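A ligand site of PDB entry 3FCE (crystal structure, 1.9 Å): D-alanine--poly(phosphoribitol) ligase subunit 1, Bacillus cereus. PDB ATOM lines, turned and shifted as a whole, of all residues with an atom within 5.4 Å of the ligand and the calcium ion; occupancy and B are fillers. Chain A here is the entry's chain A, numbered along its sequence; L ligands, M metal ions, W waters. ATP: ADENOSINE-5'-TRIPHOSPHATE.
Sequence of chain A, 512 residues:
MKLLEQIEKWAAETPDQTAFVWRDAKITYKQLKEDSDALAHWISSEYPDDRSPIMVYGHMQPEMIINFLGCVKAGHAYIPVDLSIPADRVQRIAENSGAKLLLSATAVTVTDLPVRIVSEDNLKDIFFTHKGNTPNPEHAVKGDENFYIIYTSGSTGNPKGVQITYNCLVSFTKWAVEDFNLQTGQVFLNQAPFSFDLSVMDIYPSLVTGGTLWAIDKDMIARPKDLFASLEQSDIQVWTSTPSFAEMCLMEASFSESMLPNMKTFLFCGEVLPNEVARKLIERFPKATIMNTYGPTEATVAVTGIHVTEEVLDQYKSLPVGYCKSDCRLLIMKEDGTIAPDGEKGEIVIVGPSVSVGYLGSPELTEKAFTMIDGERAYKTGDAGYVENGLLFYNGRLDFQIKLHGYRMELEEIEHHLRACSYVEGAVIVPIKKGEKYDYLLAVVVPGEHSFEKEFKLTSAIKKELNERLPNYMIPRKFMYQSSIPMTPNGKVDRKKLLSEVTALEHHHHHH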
ATOM      1  N   THR A 152       8.108   9.068  11.477  1.00  0.00           N
ATOM      2  CA  THR A 152       9.285   9.838  11.843  1.00  0.00           C
ATOM      3  C   THR A 152       9.858   9.298  13.150  1.00  0.00           C
ATOM      4  O   THR A 152       9.412   9.664  14.241  1.00  0.00           O
ATOM      5  CB  THR A 152       8.930  11.336  11.978  1.00  0.00           C
ATOM      6  OG1 THR A 152      10.089  12.070  12.411  1.00  0.00           O
ATOM      7  CG2 THR A 152       7.799  11.532  12.963  1.00  0.00           C
ATOM      8  N   SER A 153      10.866   8.426  13.011  1.00  0.00           N
ATOM      9  CA  SER A 153      11.579   7.762  14.103  1.00  0.00           C
ATOM     10  C   SER A 153      11.178   8.129  15.523  1.00  0.00           C
ATOM     11  O   SER A 153      10.565   7.321  16.226  1.00  0.00           O
ATOM     12  CB  SER A 153      13.094   7.960  13.952  1.00  0.00           C
ATOM     13  OG  SER A 153      13.454   9.319  14.151  1.00  0.00           O
ATOM     14  N   GLY A 154      11.529   9.330  15.966  1.00  0.00           N
ATOM     15  CA  GLY A 154      11.183   9.768  17.302  1.00  0.00           C
ATOM     16  C   GLY A 154      11.473   8.715  18.363  1.00  0.00           C
ATOM     17  O   GLY A 154      11.641   9.034  19.547  1.00  0.00           O
ATOM     18  N   PHE A 196      12.444   6.387   4.477  1.00  0.00           N
ATOM     19  CA  PHE A 196      12.967   7.743   4.632  1.00  0.00           C
ATOM     20  C   PHE A 196      12.419   8.480   3.411  1.00  0.00           C
ATOM     21  O   PHE A 196      12.631   8.059   2.281  1.00  0.00           O
ATOM     22  CB  PHE A 196      14.508   7.680   4.639  1.00  0.00           C
ATOM     23  CG  PHE A 196      15.190   9.014   4.762  1.00  0.00           C
ATOM     24  CD1 PHE A 196      14.564  10.109   5.352  1.00  0.00           C
ATOM     25  CD2 PHE A 196      16.504   9.164   4.325  1.00  0.00           C
ATOM     26  CE1 PHE A 196      15.228  11.320   5.503  1.00  0.00           C
ATOM     27  CE2 PHE A 196      17.183  10.366   4.465  1.00  0.00           C
ATOM     28  CZ  PHE A 196      16.542  11.444   5.050  1.00  0.00           C
ATOM     29  N   ASP A 197      11.681   9.576   3.619  1.00  0.00           N
ATOM     30  CA  ASP A 197      11.072  10.244   2.473  1.00  0.00           C
ATOM     31  C   ASP A 197      12.014  10.891   1.465  1.00  0.00           C
ATOM     32  O   ASP A 197      11.577  11.424   0.465  1.00  0.00           O
ATOM     33  CB  ASP A 197       9.997  11.252   2.915  1.00  0.00           C
ATOM     34  CG  ASP A 197      10.562  12.581   3.362  1.00  0.00           C
ATOM     35  OD1 ASP A 197       9.784  13.551   3.456  1.00  0.00           O
ATOM     36  OD2 ASP A 197      11.774  12.671   3.625  1.00  0.00           O
ATOM     37  N   PHE A 268      20.315  17.257  -3.086  1.00  0.00           N
ATOM     38  CA  PHE A 268      20.598  17.007  -1.669  1.00  0.00           C
ATOM     39  C   PHE A 268      19.493  17.512  -0.737  1.00  0.00           C
ATOM     40  O   PHE A 268      18.892  18.559  -0.970  1.00  0.00           O
ATOM     41  CB  PHE A 268      21.918  17.680  -1.289  1.00  0.00           C
ATOM     42  CG  PHE A 268      23.131  17.076  -1.946  1.00  0.00           C
ATOM     43  CD1 PHE A 268      23.539  15.782  -1.618  1.00  0.00           C
ATOM     44  CD2 PHE A 268      23.854  17.780  -2.902  1.00  0.00           C
ATOM     45  CE1 PHE A 268      24.651  15.203  -2.244  1.00  0.00           C
ATOM     46  CE2 PHE A 268      24.966  17.211  -3.538  1.00  0.00           C
ATOM     47  CZ  PHE A 268      25.367  15.921  -3.205  1.00  0.00           C
ATOM     48  N   CYS A 269      19.249  16.755   0.325  1.00  0.00           N
ATOM     49  CA  CYS A 269      18.232  17.120   1.311  1.00  0.00           C
ATOM     50  C   CYS A 269      18.475  16.313   2.583  1.00  0.00           C
ATOM     51  O   CYS A 269      19.235  15.342   2.560  1.00  0.00           O
ATOM     52  CB  CYS A 269      16.841  16.808   0.757  1.00  0.00           C
ATOM     53  SG  CYS A 269      15.477  17.552   1.676  1.00  0.00           S
ATOM     54  N   GLY A 270      17.851  16.719   3.685  1.00  0.00           N
ATOM     55  CA  GLY A 270      17.997  15.957   4.917  1.00  0.00           C
ATOM     56  C   GLY A 270      18.963  16.462   5.984  1.00  0.00           C
ATOM     57  O   GLY A 270      18.705  16.286   7.170  1.00  0.00           O
ATOM     58  N   GLU A 271      20.077  17.055   5.564  1.00  0.00           N
ATOM     59  CA  GLU A 271      21.076  17.583   6.482  1.00  0.00           C
ATOM     60  C   GLU A 271      21.758  18.796   5.871  1.00  0.00           C
ATOM     61  O   GLU A 271      21.522  19.149   4.715  1.00  0.00           O
ATOM     62  CB  GLU A 271      22.188  16.575   6.780  1.00  0.00           C
ATOM     63  CG  GLU A 271      21.853  15.123   6.586  1.00  0.00           C
ATOM     64  CD  GLU A 271      23.030  14.244   6.971  1.00  0.00           C
ATOM     65  OE1 GLU A 271      23.266  14.049   8.176  1.00  0.00           O
ATOM     66  OE2 GLU A 271      23.720  13.756   6.053  1.00  0.00           O
ATOM     67  N   VAL A 272      22.644  19.417   6.648  1.00  0.00           N
ATOM     68  CA  VAL A 272      23.414  20.550   6.172  1.00  0.00           C
ATOM     69  C   VAL A 272      24.322  20.079   5.035  1.00  0.00           C
ATOM     70  O   VAL A 272      24.975  19.039   5.141  1.00  0.00           O
ATOM     71  CB  VAL A 272      24.282  21.153   7.304  1.00  0.00           C
ATOM     72  CG1 VAL A 272      25.229  22.212   6.751  1.00  0.00           C
ATOM     73  CG2 VAL A 272      23.398  21.771   8.376  1.00  0.00           C
ATOM     74  N   LEU A 273      24.345  20.833   3.945  1.00  0.00           N
ATOM     75  CA  LEU A 273      25.209  20.524   2.814  1.00  0.00           C
ATOM     76  C   LEU A 273      26.396  21.450   2.996  1.00  0.00           C
ATOM     77  O   LEU A 273      26.283  22.658   2.802  1.00  0.00           O
ATOM     78  CB  LEU A 273      24.511  20.826   1.477  1.00  0.00           C
ATOM     79  CG  LEU A 273      25.419  20.635   0.241  1.00  0.00           C
ATOM     80  CD1 LEU A 273      25.930  19.198   0.207  1.00  0.00           C
ATOM     81  CD2 LEU A 273      24.665  20.991  -1.029  1.00  0.00           C
ATOM     82  N   ASN A 292      20.545  22.242  -3.588  1.00  0.00           N
ATOM     83  CA  ASN A 292      20.384  22.011  -2.162  1.00  0.00           C
ATOM     84  C   ASN A 292      18.900  22.281  -1.934  1.00  0.00           C
ATOM     85  O   ASN A 292      18.347  23.219  -2.500  1.00  0.00           O
ATOM     86  CB  ASN A 292      21.237  22.959  -1.324  1.00  0.00           C
ATOM     87  CG  ASN A 292      21.186  22.626   0.172  1.00  0.00           C
ATOM     88  OD1 ASN A 292      20.987  21.469   0.547  1.00  0.00           O
ATOM     89  ND2 ASN A 292      21.389  23.633   1.011  1.00  0.00           N
ATOM     90  N   THR A 293      18.254  21.439  -1.131  1.00  0.00           N
ATOM     91  CA  THR A 293      16.826  21.576  -0.840  1.00  0.00           C
ATOM     92  C   THR A 293      16.603  21.332   0.647  1.00  0.00           C
ATOM     93  O   THR A 293      17.389  20.627   1.281  1.00  0.00           O
ATOM     94  CB  THR A 293      15.985  20.553  -1.614  1.00  0.00           C
ATOM     95  OG1 THR A 293      16.286  19.225  -1.152  1.00  0.00           O
ATOM     96  CG2 THR A 293      16.294  20.632  -3.121  1.00  0.00           C
ATOM     97  N   TYR A 294      15.516  21.872   1.190  1.00  0.00           N
ATOM     98  CA  TYR A 294      15.196  21.725   2.611  1.00  0.00           C
ATOM     99  C   TYR A 294      13.727  21.441   2.863  1.00  0.00           C
ATOM    100  O   TYR A 294      12.848  21.903   2.130  1.00  0.00           O
ATOM    101  CB  TYR A 294      15.570  22.997   3.384  1.00  0.00           C
ATOM    102  CG  TYR A 294      14.782  23.170   4.685  1.00  0.00           C
ATOM    103  CD1 TYR A 294      15.248  22.633   5.881  1.00  0.00           C
ATOM    104  CD2 TYR A 294      13.560  23.845   4.691  1.00  0.00           C
ATOM    105  CE1 TYR A 294      14.508  22.759   7.060  1.00  0.00           C
ATOM    106  CE2 TYR A 294      12.808  23.977   5.867  1.00  0.00           C
ATOM    107  CZ  TYR A 294      13.295  23.426   7.048  1.00  0.00           C
ATOM    108  OH  TYR A 294      12.574  23.550   8.215  1.00  0.00           O
ATOM    109  N   GLY A 295      13.457  20.700   3.932  1.00  0.00           N
ATOM    110  CA  GLY A 295      12.085  20.405   4.287  1.00  0.00           C
ATOM    111  C   GLY A 295      11.966  19.227   5.229  1.00  0.00           C
ATOM    112  O   GLY A 295      12.851  18.376   5.289  1.00  0.00           O
ATOM    113  N   PRO A 296      10.889  19.187   6.023  1.00  0.00           N
ATOM    114  CA  PRO A 296      10.662  18.091   6.974  1.00  0.00           C
ATOM    115  C   PRO A 296       9.751  17.096   6.273  1.00  0.00           C
ATOM    116  O   PRO A 296       9.101  17.447   5.282  1.00  0.00           O
ATOM    117  CB  PRO A 296       9.953  18.790   8.116  1.00  0.00           C
ATOM    118  CG  PRO A 296       9.071  19.749   7.390  1.00  0.00           C
ATOM    119  CD  PRO A 296      10.025  20.338   6.354  1.00  0.00           C
ATOM    120  N   THR A 297       9.684  15.882   6.782  1.00  0.00           N
ATOM    121  CA  THR A 297       8.819  14.851   6.214  1.00  0.00           C
ATOM    122  C   THR A 297       7.368  15.356   6.255  1.00  0.00           C
ATOM    123  O   THR A 297       6.578  15.095   5.341  1.00  0.00           O
ATOM    124  CB  THR A 297       8.931  13.540   7.036  1.00  0.00           C
ATOM    125  OG1 THR A 297      10.274  13.056   6.983  1.00  0.00           O
ATOM    126  CG2 THR A 297       7.995  12.470   6.482  1.00  0.00           C
ATOM    127  N   GLU A 298       7.042  16.098   7.304  1.00  0.00           N
ATOM    128  CA  GLU A 298       5.708  16.652   7.517  1.00  0.00           C
ATOM    129  C   GLU A 298       5.282  17.648   6.438  1.00  0.00           C
ATOM    130  O   GLU A 298       4.134  18.094   6.410  1.00  0.00           O
ATOM    131  CB  GLU A 298       5.628  17.312   8.899  1.00  0.00           C
ATOM    132  CG  GLU A 298       5.621  16.326  10.087  1.00  0.00           C
ATOM    133  CD  GLU A 298       7.021  15.943  10.574  1.00  0.00           C
ATOM    134  OE1 GLU A 298       8.006  16.158   9.842  1.00  0.00           O
ATOM    135  OE2 GLU A 298       7.122  15.417  11.705  1.00  0.00           O
ATOM    136  N   VAL A 321      19.281  27.334   2.073  1.00  0.00           N
ATOM    137  CA  VAL A 321      18.580  26.116   1.706  1.00  0.00           C
ATOM    138  C   VAL A 321      17.586  26.279   0.570  1.00  0.00           C
ATOM    139  O   VAL A 321      16.976  25.307   0.123  1.00  0.00           O
ATOM    140  CB  VAL A 321      17.901  25.459   2.928  1.00  0.00           C
ATOM    141  CG1 VAL A 321      18.976  24.931   3.872  1.00  0.00           C
ATOM    142  CG2 VAL A 321      16.993  26.449   3.632  1.00  0.00           C
ATOM    143  N   TYR A 379       2.701  24.081   9.346  1.00  0.00           N
ATOM    144  CA  TYR A 379       3.488  23.181  10.176  1.00  0.00           C
ATOM    145  C   TYR A 379       4.706  23.873  10.803  1.00  0.00           C
ATOM    146  O   TYR A 379       5.494  24.507  10.094  1.00  0.00           O
ATOM    147  CB  TYR A 379       3.960  21.985   9.334  1.00  0.00           C
ATOM    148  CG  TYR A 379       4.869  21.037  10.067  1.00  0.00           C
ATOM    149  CD1 TYR A 379       4.398  20.291  11.155  1.00  0.00           C
ATOM    150  CD2 TYR A 379       6.220  20.906   9.706  1.00  0.00           C
ATOM    151  CE1 TYR A 379       5.256  19.449  11.878  1.00  0.00           C
ATOM    152  CE2 TYR A 379       7.085  20.058  10.423  1.00  0.00           C
ATOM    153  CZ  TYR A 379       6.587  19.338  11.509  1.00  0.00           C
ATOM    154  OH  TYR A 379       7.419  18.536  12.254  1.00  0.00           O
ATOM    155  N   THR A 381       8.217  23.616  12.112  1.00  0.00           N
ATOM    156  CA  THR A 381       9.313  22.654  11.926  1.00  0.00           C
ATOM    157  C   THR A 381      10.215  22.367  13.125  1.00  0.00           C
ATOM    158  O   THR A 381      10.825  21.295  13.181  1.00  0.00           O
ATOM    159  CB  THR A 381      10.247  23.097  10.784  1.00  0.00           C
ATOM    160  OG1 THR A 381      10.910  24.302  11.150  1.00  0.00           O
ATOM    161  CG2 THR A 381       9.460  23.315   9.478  1.00  0.00           C
ATOM    162  N   ASP A 383      12.702  24.032  13.543  1.00  0.00           N
ATOM    163  CA  ASP A 383      13.996  24.458  12.983  1.00  0.00           C
ATOM    164  C   ASP A 383      14.134  25.967  13.107  1.00  0.00           C
ATOM    165  O   ASP A 383      13.173  26.708  12.911  1.00  0.00           O
ATOM    166  CB  ASP A 383      14.080  24.087  11.499  1.00  0.00           C
ATOM    167  CG  ASP A 383      14.213  22.598  11.266  1.00  0.00           C
ATOM    168  OD1 ASP A 383      13.703  22.121  10.238  1.00  0.00           O
ATOM    169  OD2 ASP A 383      14.832  21.903  12.104  1.00  0.00           O
ATOM    170  N   TYR A 394      19.086  28.107   6.911  1.00  0.00           N
ATOM    171  CA  TYR A 394      18.937  27.170   8.016  1.00  0.00           C
ATOM    172  C   TYR A 394      20.033  27.348   9.057  1.00  0.00           C
ATOM    173  O   TYR A 394      21.224  27.284   8.724  1.00  0.00           O
ATOM    174  CB  TYR A 394      19.001  25.732   7.489  1.00  0.00           C
ATOM    175  CG  TYR A 394      18.913  24.663   8.547  1.00  0.00           C
ATOM    176  CD1 TYR A 394      17.675  24.156   8.952  1.00  0.00           C
ATOM    177  CD2 TYR A 394      20.073  24.096   9.086  1.00  0.00           C
ATOM    178  CE1 TYR A 394      17.599  23.099   9.862  1.00  0.00           C
ATOM    179  CE2 TYR A 394      20.009  23.033   9.999  1.00  0.00           C
ATOM    180  CZ  TYR A 394      18.765  22.548  10.375  1.00  0.00           C
ATOM    181  OH  TYR A 394      18.701  21.476  11.239  1.00  0.00           O
ATOM    182  N   ARG A 397      18.528  22.960  14.562  1.00  0.00           N
ATOM    183  CA  ARG A 397      17.353  22.493  15.304  1.00  0.00           C
ATOM    184  C   ARG A 397      17.280  23.200  16.653  1.00  0.00           C
ATOM    185  O   ARG A 397      18.273  23.250  17.382  1.00  0.00           O
ATOM    186  CB  ARG A 397      17.442  20.979  15.512  1.00  0.00           C
ATOM    187  CG  ARG A 397      17.392  20.146  14.245  1.00  0.00           C
ATOM    188  CD  ARG A 397      17.941  18.751  14.492  1.00  0.00           C
ATOM    189  NE  ARG A 397      18.050  17.966  13.263  1.00  0.00           N
ATOM    190  CZ  ARG A 397      17.091  17.185  12.781  1.00  0.00           C
ATOM    191  NH1 ARG A 397      15.929  17.069  13.413  1.00  0.00           N
ATOM    192  NH2 ARG A 397      17.294  16.526  11.643  1.00  0.00           N
ATOM    193  N   LYS A 492      22.298   9.363   7.329  1.00  0.00           N
ATOM    194  CA  LYS A 492      22.571  10.590   8.064  1.00  0.00           C
ATOM    195  C   LYS A 492      23.582  10.358   9.190  1.00  0.00           C
ATOM    196  O   LYS A 492      23.818   9.217   9.603  1.00  0.00           O
ATOM    197  CB  LYS A 492      21.270  11.177   8.619  1.00  0.00           C
ATOM    198  CG  LYS A 492      20.208  11.364   7.541  1.00  0.00           C
ATOM    199  CD  LYS A 492      19.090  12.298   7.952  1.00  0.00           C
ATOM    200  CE  LYS A 492      18.296  11.736   9.106  1.00  0.00           C
ATOM    201  NZ  LYS A 492      17.123  12.600   9.409  1.00  0.00           N
HETATM  202  PG  ATP L   1      13.192  12.442  13.324  1.00  0.00           P
HETATM  203  O1G ATP L   1      12.277  13.541  13.536  1.00  0.00           O
HETATM  204  O2G ATP L   1      13.607  11.888  14.658  1.00  0.00           O
HETATM  205  O3G ATP L   1      12.545  11.408  12.557  1.00  0.00           O
HETATM  206  PB  ATP L   1      14.378  14.073  11.373  1.00  0.00           P
HETATM  207  O1B ATP L   1      15.733  14.329  10.819  1.00  0.00           O
HETATM  208  O2B ATP L   1      13.856  15.293  11.953  1.00  0.00           O
HETATM  209  O3B ATP L   1      14.501  12.952  12.516  1.00  0.00           O
HETATM  210  PA  ATP L   1      13.312  14.277   8.725  1.00  0.00           P
HETATM  211  O1A ATP L   1      13.620  13.218   7.650  1.00  0.00           O
HETATM  212  O2A ATP L   1      11.953  14.801   8.509  1.00  0.00           O
HETATM  213  O3A ATP L   1      13.395  13.558  10.196  1.00  0.00           O
HETATM  214  O5' ATP L   1      14.423  15.507   8.585  1.00  0.00           O
HETATM  215  C5' ATP L   1      13.985  16.971   8.541  1.00  0.00           C
HETATM  216  C4' ATP L   1      14.888  17.727   9.162  1.00  0.00           C
HETATM  217  O4' ATP L   1      16.201  17.626   8.472  1.00  0.00           O
HETATM  218  C3' ATP L   1      14.501  19.245   9.119  1.00  0.00           C
HETATM  219  O3' ATP L   1      13.595  19.572  10.100  1.00  0.00           O
HETATM  220  C2' ATP L   1      15.912  19.947   9.100  1.00  0.00           C
HETATM  221  O2' ATP L   1      16.380  20.109  10.547  1.00  0.00           O
HETATM  222  C1' ATP L   1      16.823  18.934   8.402  1.00  0.00           C
HETATM  223  N9  ATP L   1      17.093  19.316   7.122  1.00  0.00           N
HETATM  224  C8  ATP L   1      16.397  18.948   5.953  1.00  0.00           C
HETATM  225  N7  ATP L   1      16.961  19.516   4.922  1.00  0.00           N
HETATM  226  C5  ATP L   1      18.015  20.248   5.348  1.00  0.00           C
HETATM  227  C6  ATP L   1      18.969  21.048   4.715  1.00  0.00           C
HETATM  228  N6  ATP L   1      18.960  21.224   3.376  1.00  0.00           N
HETATM  229  N1  ATP L   1      19.960  21.681   5.488  1.00  0.00           N
HETATM  230  C2  ATP L   1      19.996  21.515   6.895  1.00  0.00           C
HETATM  231  N3  ATP L   1      19.082  20.744   7.555  1.00  0.00           N
HETATM  232  C4  ATP L   1      18.101  20.119   6.730  1.00  0.00           C
HETATM  233 CA    CA M   1      11.696  15.926  12.772  1.00  0.00          CA
HETATM  234  O   HOH W   1      14.564  16.418   4.582  1.00  0.00           O
HETATM  235  O   HOH W   2      22.181  22.765   4.003  1.00  0.00           O
HETATM  236  O   HOH W   3      17.408  13.151  13.109  1.00  0.00           O
HETATM  237  O   HOH W   4      12.677  18.211  12.305  1.00  0.00           O
HETATM  238  O   HOH W   5      12.652  16.714  14.737  1.00  0.00           O
HETATM  239  O   HOH W   6      20.860  18.866   1.963  1.00  0.00           O
HETATM  240  O   HOH W   7       9.387  15.467  13.073  1.00  0.00           O
HETATM  241  O   HOH W   8      10.762  15.978  10.554  1.00  0.00           O
HETATM  242  O   HOH W   9      10.419  19.191  11.451  1.00  0.00           O
HETATM  243  O   HOH W  10      15.934  10.997  13.668  1.00  0.00           O
HETATM  244  O   HOH W  11      10.928  12.868  16.372  1.00  0.00           O
HETATM  245  O   HOH W  12      16.618  14.254   7.361  1.00  0.00           O
HETATM  246  O   HOH W  13      20.555  19.309   9.670  1.00  0.00           O
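O3G of the ligand is in hydrogen-bond range of OG1 of Thr 152, at 2.5 Å. O3' of the ligand lies within hydrogen-bond range of OD1 of Asp 383, 2.6 Å away. N of Ser 153 is in hydrogen-bond range of O3G of the ligand (3.5 Å). The side-chain hydroxyl (OG) of Ser 153 sits at hydrogen-bond distance from an oxygen (O2G) of the ligand. NZ of Lys 492 is in salt-bridge range of O1B of the ligand. The backbone carbonyl oxygen of Thr 293 lies within hydrogen-bond range of a nitrogen (N6) of the ligand. The side-chain hydroxyl of Tyr 394 sits at hydrogen-bond distance from an oxygen (O2') of the ligand (2.8 Å). An oxygen (O1B) of the ligand lies within salt-bridge range of the guanidinium group of Arg 397 (2.8 Å). N of Thr 297 sits at hydrogen-bond distance from O2A of the ligand (3.0 Å). An oxygen (O2A) of the ligand lies within hydrogen-bond range of the side-chain hydroxyl (OG1) of Thr 297 (2.9 Å). A nitrogen (N7) of the ligand is in hydrogen-bond range of the backbone NH (N) of Gly 270, at 3.2 Å. A nitrogen (N6) of the ligand is in hydrogen-bond range of the side-chain amide oxygen (OD1) of Asn 292 (3.5 Å).
The side-chain carboxylate (OD1) of Asp 383 is in hydrogen-bond range of the side-chain hydroxyl (OH) of Tyr 294 (2.7 Å). The side-chain hydroxyl (OG1) of Thr 381 sits at hydrogen-bond distance from the backbone NH (N) of Asp 383 (3.0 Å). OG1 of Thr 293 sits close to SG of Cys 269, at 3.4 Å. OG1 of Thr 293 sits at hydrogen-bond distance from O of Phe 268. OH of Tyr 294 lies close to OG1 of Thr 381 (3.5 Å).
A nitrogen (N1) of the ligand lies close to the backbone carbonyl oxygen (O) of Glu 271 (3.1 Å). Merely in contact with the ligand: Phe 196, Val 272, Gly 154, Tyr 294, Gly 295, Val 321 and Pro 296. Of the 25 residues printed, 18 come within 4 Å of the ligand. The nearest printed residue that does not touch the ligand is Cys 269 (4.1 Å).
No residue comes within 4 Å of the calcium ion.
Water W5 is bound to the calcium ion (2.3 Å). Water W7 is bound to the calcium ion (2.4 Å). An oxygen (O2B) of the ligand binds the calcium ion. The calcium ion is bound by water W8, at 2.4 Å. Water W4 binds the calcium ion (2.5 Å). O1G of the ligand is bound to the calcium ion (2.6 Å).
Water W8 bridges an oxygen (O2A) of the ligand (2.6 Å) and the side-chain carboxylate (OE1) of Glu 298 (2.9 Å). Water W10 bridges an oxygen (O2G) of the ligand (2.7 Å) and the side-chain hydroxyl (OG) of Ser 153 (3.0 Å). Water W12 lies within hydrogen-bond range of the side-chain amino group of Lys 492 (2.7 Å), an oxygen (O5') of the ligand (2.8 Å) and the backbone carbonyl oxygen of Gly 270 (2.9 Å). Water W2 lies within hydrogen-bond range of N1 of the ligand (2.9 Å), N of Leu 273 (2.9 Å) and ND2 of Asn 292 (3.2 Å). Water W6 lies within hydrogen-bond range of O of Glu 271 (2.8 Å), OD1 of Asn 292 (3.0 Å), N of Cys 269 (3.1 Å) and N6 of the ligand (3.3 Å). Water W9 lies within hydrogen-bond range of O of Thr 381, OH of Tyr 379 and O3' of the ligand.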
